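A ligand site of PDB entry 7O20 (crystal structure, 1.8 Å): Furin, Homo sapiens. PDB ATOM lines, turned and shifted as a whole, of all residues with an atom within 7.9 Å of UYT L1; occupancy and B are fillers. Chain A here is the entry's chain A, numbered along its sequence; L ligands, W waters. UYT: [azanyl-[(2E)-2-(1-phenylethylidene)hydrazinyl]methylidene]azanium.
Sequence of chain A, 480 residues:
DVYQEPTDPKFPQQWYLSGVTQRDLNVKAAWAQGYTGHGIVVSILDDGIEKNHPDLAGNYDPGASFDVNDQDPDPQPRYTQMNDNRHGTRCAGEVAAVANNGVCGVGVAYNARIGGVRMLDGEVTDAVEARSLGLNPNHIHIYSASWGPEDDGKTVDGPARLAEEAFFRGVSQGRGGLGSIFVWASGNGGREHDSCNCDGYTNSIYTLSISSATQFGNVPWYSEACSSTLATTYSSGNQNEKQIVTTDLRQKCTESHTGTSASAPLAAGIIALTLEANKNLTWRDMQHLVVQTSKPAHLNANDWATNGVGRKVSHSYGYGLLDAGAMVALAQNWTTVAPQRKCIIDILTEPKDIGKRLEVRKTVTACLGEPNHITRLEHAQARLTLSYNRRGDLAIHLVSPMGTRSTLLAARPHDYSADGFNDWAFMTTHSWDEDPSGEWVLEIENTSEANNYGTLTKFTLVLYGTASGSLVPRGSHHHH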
ATOM      1  N   MET A 119      -0.544  17.727  18.556  1.00  0.00           N
ATOM      2  CA  MET A 119      -1.194  18.058  19.818  1.00  0.00           C
ATOM      3  C   MET A 119      -2.722  18.050  19.788  1.00  0.00           C
ATOM      4  O   MET A 119      -3.324  18.089  20.853  1.00  0.00           O
ATOM      5  CB  MET A 119      -0.694  19.427  20.319  1.00  0.00           C
ATOM      6  CG  MET A 119      -0.614  20.519  19.281  1.00  0.00           C
ATOM      7  SD  MET A 119      -2.188  21.359  19.000  1.00  0.00           S
ATOM      8  CE  MET A 119      -2.573  22.034  20.616  1.00  0.00           C
ATOM      9  N   LEU A 120      -3.373  17.883  18.637  1.00  0.00           N
ATOM     10  CA  LEU A 120      -4.823  17.836  18.608  1.00  0.00           C
ATOM     11  C   LEU A 120      -5.379  16.413  18.629  1.00  0.00           C
ATOM     12  O   LEU A 120      -6.598  16.260  18.788  1.00  0.00           O
ATOM     13  CB  LEU A 120      -5.347  18.529  17.349  1.00  0.00           C
ATOM     14  CG  LEU A 120      -5.164  20.045  17.245  1.00  0.00           C
ATOM     15  CD1 LEU A 120      -5.697  20.574  15.915  1.00  0.00           C
ATOM     16  CD2 LEU A 120      -5.841  20.732  18.429  1.00  0.00           C
ATOM     17  N   GLY A 122      -5.844  13.761  20.587  1.00  0.00           N
ATOM     18  CA  GLY A 122      -5.849  13.367  21.982  1.00  0.00           C
ATOM     19  C   GLY A 122      -6.667  14.370  22.781  1.00  0.00           C
ATOM     20  O   GLY A 122      -7.254  15.292  22.221  1.00  0.00           O
ATOM     21  N   GLU A 123      -6.657  14.193  24.092  1.00  0.00           N
ATOM     22  CA  GLU A 123      -7.352  15.121  24.965  1.00  0.00           C
ATOM     23  C   GLU A 123      -6.552  16.429  25.006  1.00  0.00           C
ATOM     24  O   GLU A 123      -5.379  16.438  25.412  1.00  0.00           O
ATOM     25  CB  GLU A 123      -7.483  14.504  26.356  1.00  0.00           C
ATOM     26  CG  GLU A 123      -8.527  15.193  27.225  1.00  0.00           C
ATOM     27  N   VAL A 124      -7.154  17.537  24.581  1.00  0.00           N
ATOM     28  CA  VAL A 124      -6.445  18.816  24.470  1.00  0.00           C
ATOM     29  C   VAL A 124      -6.727  19.607  25.739  1.00  0.00           C
ATOM     30  O   VAL A 124      -7.701  20.379  25.823  1.00  0.00           O
ATOM     31  CB  VAL A 124      -6.830  19.596  23.218  1.00  0.00           C
ATOM     32  CG1 VAL A 124      -5.997  20.899  23.142  1.00  0.00           C
ATOM     33  CG2 VAL A 124      -6.655  18.726  21.978  1.00  0.00           C
ATOM     34  N   THR A 125      -5.848  19.461  26.721  1.00  0.00           N
ATOM     35  CA  THR A 125      -5.912  20.179  27.971  1.00  0.00           C
ATOM     36  C   THR A 125      -5.146  21.486  27.888  1.00  0.00           C
ATOM     37  O   THR A 125      -4.410  21.749  26.949  1.00  0.00           O
ATOM     38  CB  THR A 125      -5.267  19.347  29.087  1.00  0.00           C
ATOM     39  OG1 THR A 125      -3.886  19.139  28.707  1.00  0.00           O
ATOM     40  CG2 THR A 125      -5.966  18.011  29.250  1.00  0.00           C
ATOM     41  N   ASP A 126      -5.281  22.290  28.946  1.00  0.00           N
ATOM     42  CA  ASP A 126      -4.495  23.524  29.071  1.00  0.00           C
ATOM     43  C   ASP A 126      -2.998  23.203  29.009  1.00  0.00           C
ATOM     44  O   ASP A 126      -2.243  23.897  28.320  1.00  0.00           O
ATOM     45  CB  ASP A 126      -4.919  24.205  30.390  1.00  0.00           C
ATOM     46  CG  ASP A 126      -4.180  25.510  30.693  1.00  0.00           C
ATOM     47  OD1 ASP A 126      -3.960  26.313  29.778  1.00  0.00           O
ATOM     48  OD2 ASP A 126      -3.891  25.740  31.903  1.00  0.00           O
ATOM     49  N   GLU A 129      -1.937  22.465  25.373  1.00  0.00           N
ATOM     50  CA  GLU A 129      -1.808  23.723  24.617  1.00  0.00           C
ATOM     51  C   GLU A 129      -0.537  24.465  24.985  1.00  0.00           C
ATOM     52  O   GLU A 129       0.170  24.991  24.108  1.00  0.00           O
ATOM     53  CB  GLU A 129      -3.022  24.621  24.857  1.00  0.00           C
ATOM     54  CG  GLU A 129      -4.339  23.998  24.441  1.00  0.00           C
ATOM     55  CD  GLU A 129      -5.528  24.893  24.747  1.00  0.00           C
ATOM     56  OE1 GLU A 129      -5.355  26.030  25.206  1.00  0.00           O
ATOM     57  OE2 GLU A 129      -6.662  24.428  24.549  1.00  0.00           O
ATOM     58  N   SER A 146      -4.969  26.994  14.378  1.00  0.00           N
ATOM     59  CA  SER A 146      -6.350  27.351  14.048  1.00  0.00           C
ATOM     60  C   SER A 146      -7.355  26.709  14.995  1.00  0.00           C
ATOM     61  O   SER A 146      -8.545  26.666  14.688  1.00  0.00           O
ATOM     62  CB  SER A 146      -6.662  26.974  12.595  1.00  0.00           C
ATOM     63  OG  SER A 146      -6.286  25.647  12.335  1.00  0.00           O
ATOM     64  N   TRP A 147      -6.896  26.258  16.156  1.00  0.00           N
ATOM     65  CA  TRP A 147      -7.757  25.686  17.160  1.00  0.00           C
ATOM     66  C   TRP A 147      -8.148  26.709  18.220  1.00  0.00           C
ATOM     67  O   TRP A 147      -7.548  27.791  18.351  1.00  0.00           O
ATOM     68  CB  TRP A 147      -7.076  24.465  17.810  1.00  0.00           C
ATOM     69  CG  TRP A 147      -5.602  24.591  18.070  1.00  0.00           C
ATOM     70  CD1 TRP A 147      -4.572  24.220  17.229  1.00  0.00           C
ATOM     71  CD2 TRP A 147      -4.973  25.094  19.258  1.00  0.00           C
ATOM     72  NE1 TRP A 147      -3.365  24.465  17.837  1.00  0.00           N
ATOM     73  CE2 TRP A 147      -3.585  25.026  19.053  1.00  0.00           C
ATOM     74  CE3 TRP A 147      -5.451  25.608  20.449  1.00  0.00           C
ATOM     75  CZ2 TRP A 147      -2.678  25.433  20.035  1.00  0.00           C
ATOM     76  CZ3 TRP A 147      -4.560  26.000  21.403  1.00  0.00           C
ATOM     77  CH2 TRP A 147      -3.183  25.913  21.203  1.00  0.00           C
ATOM     78  N   GLY A 148      -9.130  26.342  19.015  1.00  0.00           N
ATOM     79  CA  GLY A 148      -9.752  27.240  19.955  1.00  0.00           C
ATOM     80  C   GLY A 148     -11.040  26.607  20.426  1.00  0.00           C
ATOM     81  O   GLY A 148     -11.284  25.403  20.196  1.00  0.00           O
ATOM     82  N   PRO A 149     -11.891  27.381  21.077  1.00  0.00           N
ATOM     83  CA  PRO A 149     -13.131  26.818  21.605  1.00  0.00           C
ATOM     84  C   PRO A 149     -14.098  26.467  20.479  1.00  0.00           C
ATOM     85  O   PRO A 149     -13.975  26.924  19.352  1.00  0.00           O
ATOM     86  CB  PRO A 149     -13.718  27.939  22.470  1.00  0.00           C
ATOM     87  CG  PRO A 149     -12.744  29.109  22.383  1.00  0.00           C
ATOM     88  CD  PRO A 149     -11.793  28.858  21.278  1.00  0.00           C
ATOM     89  N   GLU A 150     -15.073  25.624  20.816  1.00  0.00           N
ATOM     90  CA  GLU A 150     -16.047  25.182  19.843  1.00  0.00           C
ATOM     91  C   GLU A 150     -16.630  26.365  19.086  1.00  0.00           C
ATOM     92  O   GLU A 150     -16.977  27.384  19.674  1.00  0.00           O
ATOM     93  CB  GLU A 150     -17.181  24.413  20.535  1.00  0.00           C
ATOM     94  CG  GLU A 150     -16.753  23.082  21.124  1.00  0.00           C
ATOM     95  CD  GLU A 150     -16.404  22.061  20.077  1.00  0.00           C
ATOM     96  OE1 GLU A 150     -15.567  21.171  20.358  1.00  0.00           O
ATOM     97  OE2 GLU A 150     -16.964  22.147  18.955  1.00  0.00           O
ATOM     98  N   ASP A 151     -16.738  26.215  17.770  1.00  0.00           N
ATOM     99  CA  ASP A 151     -17.341  27.239  16.921  1.00  0.00           C
ATOM    100  C   ASP A 151     -18.844  27.016  16.805  1.00  0.00           C
ATOM    101  O   ASP A 151     -19.405  26.980  15.702  1.00  0.00           O
ATOM    102  CB  ASP A 151     -16.682  27.228  15.549  1.00  0.00           C
ATOM    103  CG  ASP A 151     -15.322  27.908  15.546  1.00  0.00           C
ATOM    104  OD1 ASP A 151     -15.064  28.760  16.431  1.00  0.00           O
ATOM    105  OD2 ASP A 151     -14.525  27.588  14.642  1.00  0.00           O
ATOM    106  N   THR A 155     -20.339  29.563  22.717  1.00  0.00           N
ATOM    107  CA  THR A 155     -19.276  29.373  23.676  1.00  0.00           C
ATOM    108  C   THR A 155     -18.504  30.674  23.862  1.00  0.00           C
ATOM    109  O   THR A 155     -18.243  31.392  22.893  1.00  0.00           O
ATOM    110  CB  THR A 155     -18.340  28.278  23.185  1.00  0.00           C
ATOM    111  OG1 THR A 155     -19.041  27.023  23.084  1.00  0.00           O
ATOM    112  CG2 THR A 155     -17.152  28.083  24.105  1.00  0.00           C
ATOM    113  N   VAL A 156     -18.155  30.978  25.110  1.00  0.00           N
ATOM    114  CA  VAL A 156     -17.210  32.061  25.414  1.00  0.00           C
ATOM    115  C   VAL A 156     -16.091  31.399  26.202  1.00  0.00           C
ATOM    116  O   VAL A 156     -16.316  30.962  27.336  1.00  0.00           O
ATOM    117  CB  VAL A 156     -17.809  33.210  26.230  1.00  0.00           C
ATOM    118  CG1 VAL A 156     -16.731  34.310  26.426  1.00  0.00           C
ATOM    119  CG2 VAL A 156     -19.005  33.818  25.551  1.00  0.00           C
ATOM    120  N   ASP A 157     -14.903  31.296  25.604  1.00  0.00           N
ATOM    121  CA  ASP A 157     -13.805  30.614  26.276  1.00  0.00           C
ATOM    122  C   ASP A 157     -12.524  31.017  25.581  1.00  0.00           C
ATOM    123  O   ASP A 157     -12.525  31.547  24.475  1.00  0.00           O
ATOM    124  CB  ASP A 157     -13.986  29.091  26.250  1.00  0.00           C
ATOM    125  CG  ASP A 157     -13.125  28.364  27.310  1.00  0.00           C
ATOM    126  OD1 ASP A 157     -12.554  28.994  28.242  1.00  0.00           O
ATOM    127  OD2 ASP A 157     -13.080  27.147  27.207  1.00  0.00           O
ATOM    128  N   GLY A 158     -11.411  30.810  26.285  1.00  0.00           N
ATOM    129  CA  GLY A 158     -10.101  31.130  25.749  1.00  0.00           C
ATOM    130  C   GLY A 158      -9.019  30.370  26.482  1.00  0.00           C
ATOM    131  O   GLY A 158      -9.296  29.418  27.218  1.00  0.00           O
ATOM    132  N   PRO A 159      -7.774  30.780  26.316  1.00  0.00           N
ATOM    133  CA  PRO A 159      -6.679  30.061  26.986  1.00  0.00           C
ATOM    134  C   PRO A 159      -6.855  30.087  28.502  1.00  0.00           C
ATOM    135  O   PRO A 159      -7.172  31.116  29.110  1.00  0.00           O
ATOM    136  CB  PRO A 159      -5.425  30.807  26.536  1.00  0.00           C
ATOM    137  CG  PRO A 159      -5.872  32.136  26.056  1.00  0.00           C
ATOM    138  CD  PRO A 159      -7.283  31.906  25.489  1.00  0.00           C
ATOM    139  N   ALA A 160      -6.666  28.930  29.115  1.00  0.00           N
ATOM    140  CA  ALA A 160      -6.608  28.876  30.575  1.00  0.00           C
ATOM    141  C   ALA A 160      -5.199  29.308  31.030  1.00  0.00           C
ATOM    142  O   ALA A 160      -4.398  29.825  30.242  1.00  0.00           O
ATOM    143  CB  ALA A 160      -7.012  27.490  31.061  1.00  0.00           C
ATOM    144  N   ALA A 163      -1.792  28.108  29.211  1.00  0.00           N
ATOM    145  CA  ALA A 163      -1.689  28.607  27.850  1.00  0.00           C
ATOM    146  C   ALA A 163      -1.503  30.121  27.810  1.00  0.00           C
ATOM    147  O   ALA A 163      -0.754  30.660  26.980  1.00  0.00           O
ATOM    148  CB  ALA A 163      -2.933  28.219  27.054  1.00  0.00           C
ATOM    149  N   TRP A 184      -2.766  33.121  13.942  1.00  0.00           N
ATOM    150  CA  TRP A 184      -3.962  32.428  14.393  1.00  0.00           C
ATOM    151  C   TRP A 184      -5.103  32.628  13.406  1.00  0.00           C
ATOM    152  O   TRP A 184      -5.275  33.723  12.850  1.00  0.00           O
ATOM    153  CB  TRP A 184      -4.437  32.929  15.781  1.00  0.00           C
ATOM    154  CG  TRP A 184      -4.945  31.840  16.626  1.00  0.00           C
ATOM    155  CD1 TRP A 184      -6.210  31.327  16.651  1.00  0.00           C
ATOM    156  CD2 TRP A 184      -4.178  31.069  17.551  1.00  0.00           C
ATOM    157  NE1 TRP A 184      -6.266  30.259  17.540  1.00  0.00           N
ATOM    158  CE2 TRP A 184      -5.029  30.087  18.097  1.00  0.00           C
ATOM    159  CE3 TRP A 184      -2.842  31.119  17.974  1.00  0.00           C
ATOM    160  CZ2 TRP A 184      -4.605  29.188  19.074  1.00  0.00           C
ATOM    161  CZ3 TRP A 184      -2.417  30.204  18.938  1.00  0.00           C
ATOM    162  CH2 TRP A 184      -3.282  29.259  19.472  1.00  0.00           C
ATOM    163  N   ASP A 199     -13.754  34.070  21.335  1.00  0.00           N
ATOM    164  CA  ASP A 199     -12.685  33.068  21.275  1.00  0.00           C
ATOM    165  C   ASP A 199     -11.441  33.765  21.803  1.00  0.00           C
ATOM    166  O   ASP A 199     -10.891  34.628  21.114  1.00  0.00           O
ATOM    167  CB  ASP A 199     -12.552  32.569  19.832  1.00  0.00           C
ATOM    168  CG  ASP A 199     -11.247  31.841  19.503  1.00  0.00           C
ATOM    169  OD1 ASP A 199     -10.288  31.772  20.320  1.00  0.00           O
ATOM    170  OD2 ASP A 199     -11.174  31.324  18.356  1.00  0.00           O
ATOM    171  N   GLY A 200     -11.016  33.412  23.018  1.00  0.00           N
ATOM    172  CA  GLY A 200      -9.922  34.130  23.672  1.00  0.00           C
ATOM    173  C   GLY A 200      -8.569  33.937  23.028  1.00  0.00           C
ATOM    174  O   GLY A 200      -7.639  34.706  23.314  1.00  0.00           O
ATOM    175  N   TYR A 201      -8.428  32.938  22.153  1.00  0.00           N
ATOM    176  CA  TYR A 201      -7.155  32.748  21.457  1.00  0.00           C
ATOM    177  C   TYR A 201      -7.005  33.796  20.363  1.00  0.00           C
ATOM    178  O   TYR A 201      -6.034  34.545  20.335  1.00  0.00           O
ATOM    179  CB  TYR A 201      -7.038  31.326  20.874  1.00  0.00           C
ATOM    180  CG  TYR A 201      -7.128  30.261  21.927  1.00  0.00           C
ATOM    181  CD1 TYR A 201      -8.353  29.839  22.400  1.00  0.00           C
ATOM    182  CD2 TYR A 201      -5.976  29.682  22.482  1.00  0.00           C
ATOM    183  CE1 TYR A 201      -8.457  28.880  23.406  1.00  0.00           C
ATOM    184  CE2 TYR A 201      -6.083  28.709  23.505  1.00  0.00           C
ATOM    185  CZ  TYR A 201      -7.325  28.309  23.935  1.00  0.00           C
ATOM    186  OH  TYR A 201      -7.488  27.329  24.920  1.00  0.00           O
HETATM  187  CAA UYT L   1      -8.308  24.000  22.213  1.00  0.00           C
HETATM  188  CAB UYT L   1      -9.757  23.680  22.502  1.00  0.00           C
HETATM  189  CAE UYT L   1     -10.626  25.868  25.129  1.00  0.00           C
HETATM  190  CAH UYT L   1     -10.411  22.667  21.798  1.00  0.00           C
HETATM  191  CAI UYT L   1     -11.800  22.595  21.769  1.00  0.00           C
HETATM  192  CAJ UYT L   1     -12.418  21.551  21.085  1.00  0.00           C
HETATM  193  CAK UYT L   1     -11.647  20.558  20.459  1.00  0.00           C
HETATM  194  CAL UYT L   1     -10.258  20.607  20.516  1.00  0.00           C
HETATM  195  CAM UYT L   1      -9.638  21.672  21.189  1.00  0.00           C
HETATM  196  NAC UYT L   1     -10.431  24.315  23.470  1.00  0.00           N
HETATM  197  NAD UYT L   1      -9.833  25.274  24.220  1.00  0.00           N
HETATM  198  NAF UYT L   1     -11.925  25.534  25.251  1.00  0.00           N
HETATM  199  NAG UYT L   1     -10.117  26.770  25.959  1.00  0.00           N
HETATM  200  CAA UYT L   2     -13.097  23.980  17.912  1.00  0.00           C
HETATM  201  CAB UYT L   2     -11.858  24.174  17.030  1.00  0.00           C
HETATM  202  CAE UYT L   2     -11.581  27.682  17.064  1.00  0.00           C
HETATM  203  CAH UYT L   2     -11.113  23.080  16.611  1.00  0.00           C
HETATM  204  CAI UYT L   2     -10.129  23.219  15.668  1.00  0.00           C
HETATM  205  CAJ UYT L   2      -9.364  22.109  15.267  1.00  0.00           C
HETATM  206  CAK UYT L   2      -9.584  20.861  15.858  1.00  0.00           C
HETATM  207  CAL UYT L   2     -10.558  20.732  16.836  1.00  0.00           C
HETATM  208  CAM UYT L   2     -11.308  21.844  17.234  1.00  0.00           C
HETATM  209  NAC UYT L   2     -11.387  25.391  16.772  1.00  0.00           N
HETATM  210  NAD UYT L   2     -12.048  26.448  17.327  1.00  0.00           N
HETATM  211  NAF UYT L   2     -10.500  27.893  16.299  1.00  0.00           N
HETATM  212  NAG UYT L   2     -12.218  28.675  17.663  1.00  0.00           N
HETATM  213  O   HOH W   1     -14.892  24.579  23.800  1.00  0.00           O
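The side-chain carboxylate (OD2) of Asp 157 lies within salt-bridge range of a nitrogen (NAF) of UYT L1, 2.8 Å away.
A nitrogen (NAG) of UYT L1 is in hydrogen-bond range of the side-chain hydroxyl (OH) of Tyr 201, at 2.9 Å.
OE2 of Glu 129 lies close to NAD of UYT L1 (3.3 Å).
The backbone carbonyl oxygen (O) of Gly 158 lies within hydrogen-bond range of a nitrogen (NAG) of UYT L1 (3.0 Å).
The backbone NH of Gly 148 is in hydrogen-bond range of a nitrogen (NAC) of UYT L2 (3.3 Å).
The backbone carbonyl oxygen (O) of Gly 148 sits close to a nitrogen (NAD) of UYT L2 (3.1 Å).
The backbone carbonyl oxygen of Pro 149 lies within hydrogen-bond range of a nitrogen (NAG) of UYT L2 (3.0 Å).
The side-chain carboxylate of Asp 151 lies within salt-bridge range of a nitrogen (NAG) of UYT L2, at 3.95 Å.
NAG of UYT L2 is in salt-bridge range of OD2 of Asp 199 (2.9 Å).
O of Ser 146 lies within hydrogen-bond range of NAF of UYT L2.
The backbone carbonyl oxygen (O) of Asp 157 is in hydrogen-bond range of the backbone NH (N) of Gly 200.
OH of Tyr 201 is in hydrogen-bond range of OE1 of Glu 129 (2.5 Å).
OD1 of Asp 199 lies within hydrogen-bond range of N of Tyr 201 (2.9 Å).
The indole nitrogen of Trp 147 sits at hydrogen-bond distance from the side-chain sulfur of Met 119, 3.5 Å away.
NE1 of Trp 184 is in hydrogen-bond range of O of Trp 147 (2.9 Å).
Residues that only touch UYT L1: Glu 150, Gly 148, Trp 147 and Val 124.
Hydrophobic or aromatic side chains within 4 Å of UYT L1: Val 124, Trp 147 and Tyr 201.
Eight residues have an atom within 4 Å of UYT L1: Val 124, Glu 129, Trp 147, Gly 148, Glu 150, Asp 157, Gly 158 and Tyr 201.
Water W1 lies within hydrogen-bond range of N of Glu 150 (3.2 Å) and NAF of UYT L1 (3.4 Å).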
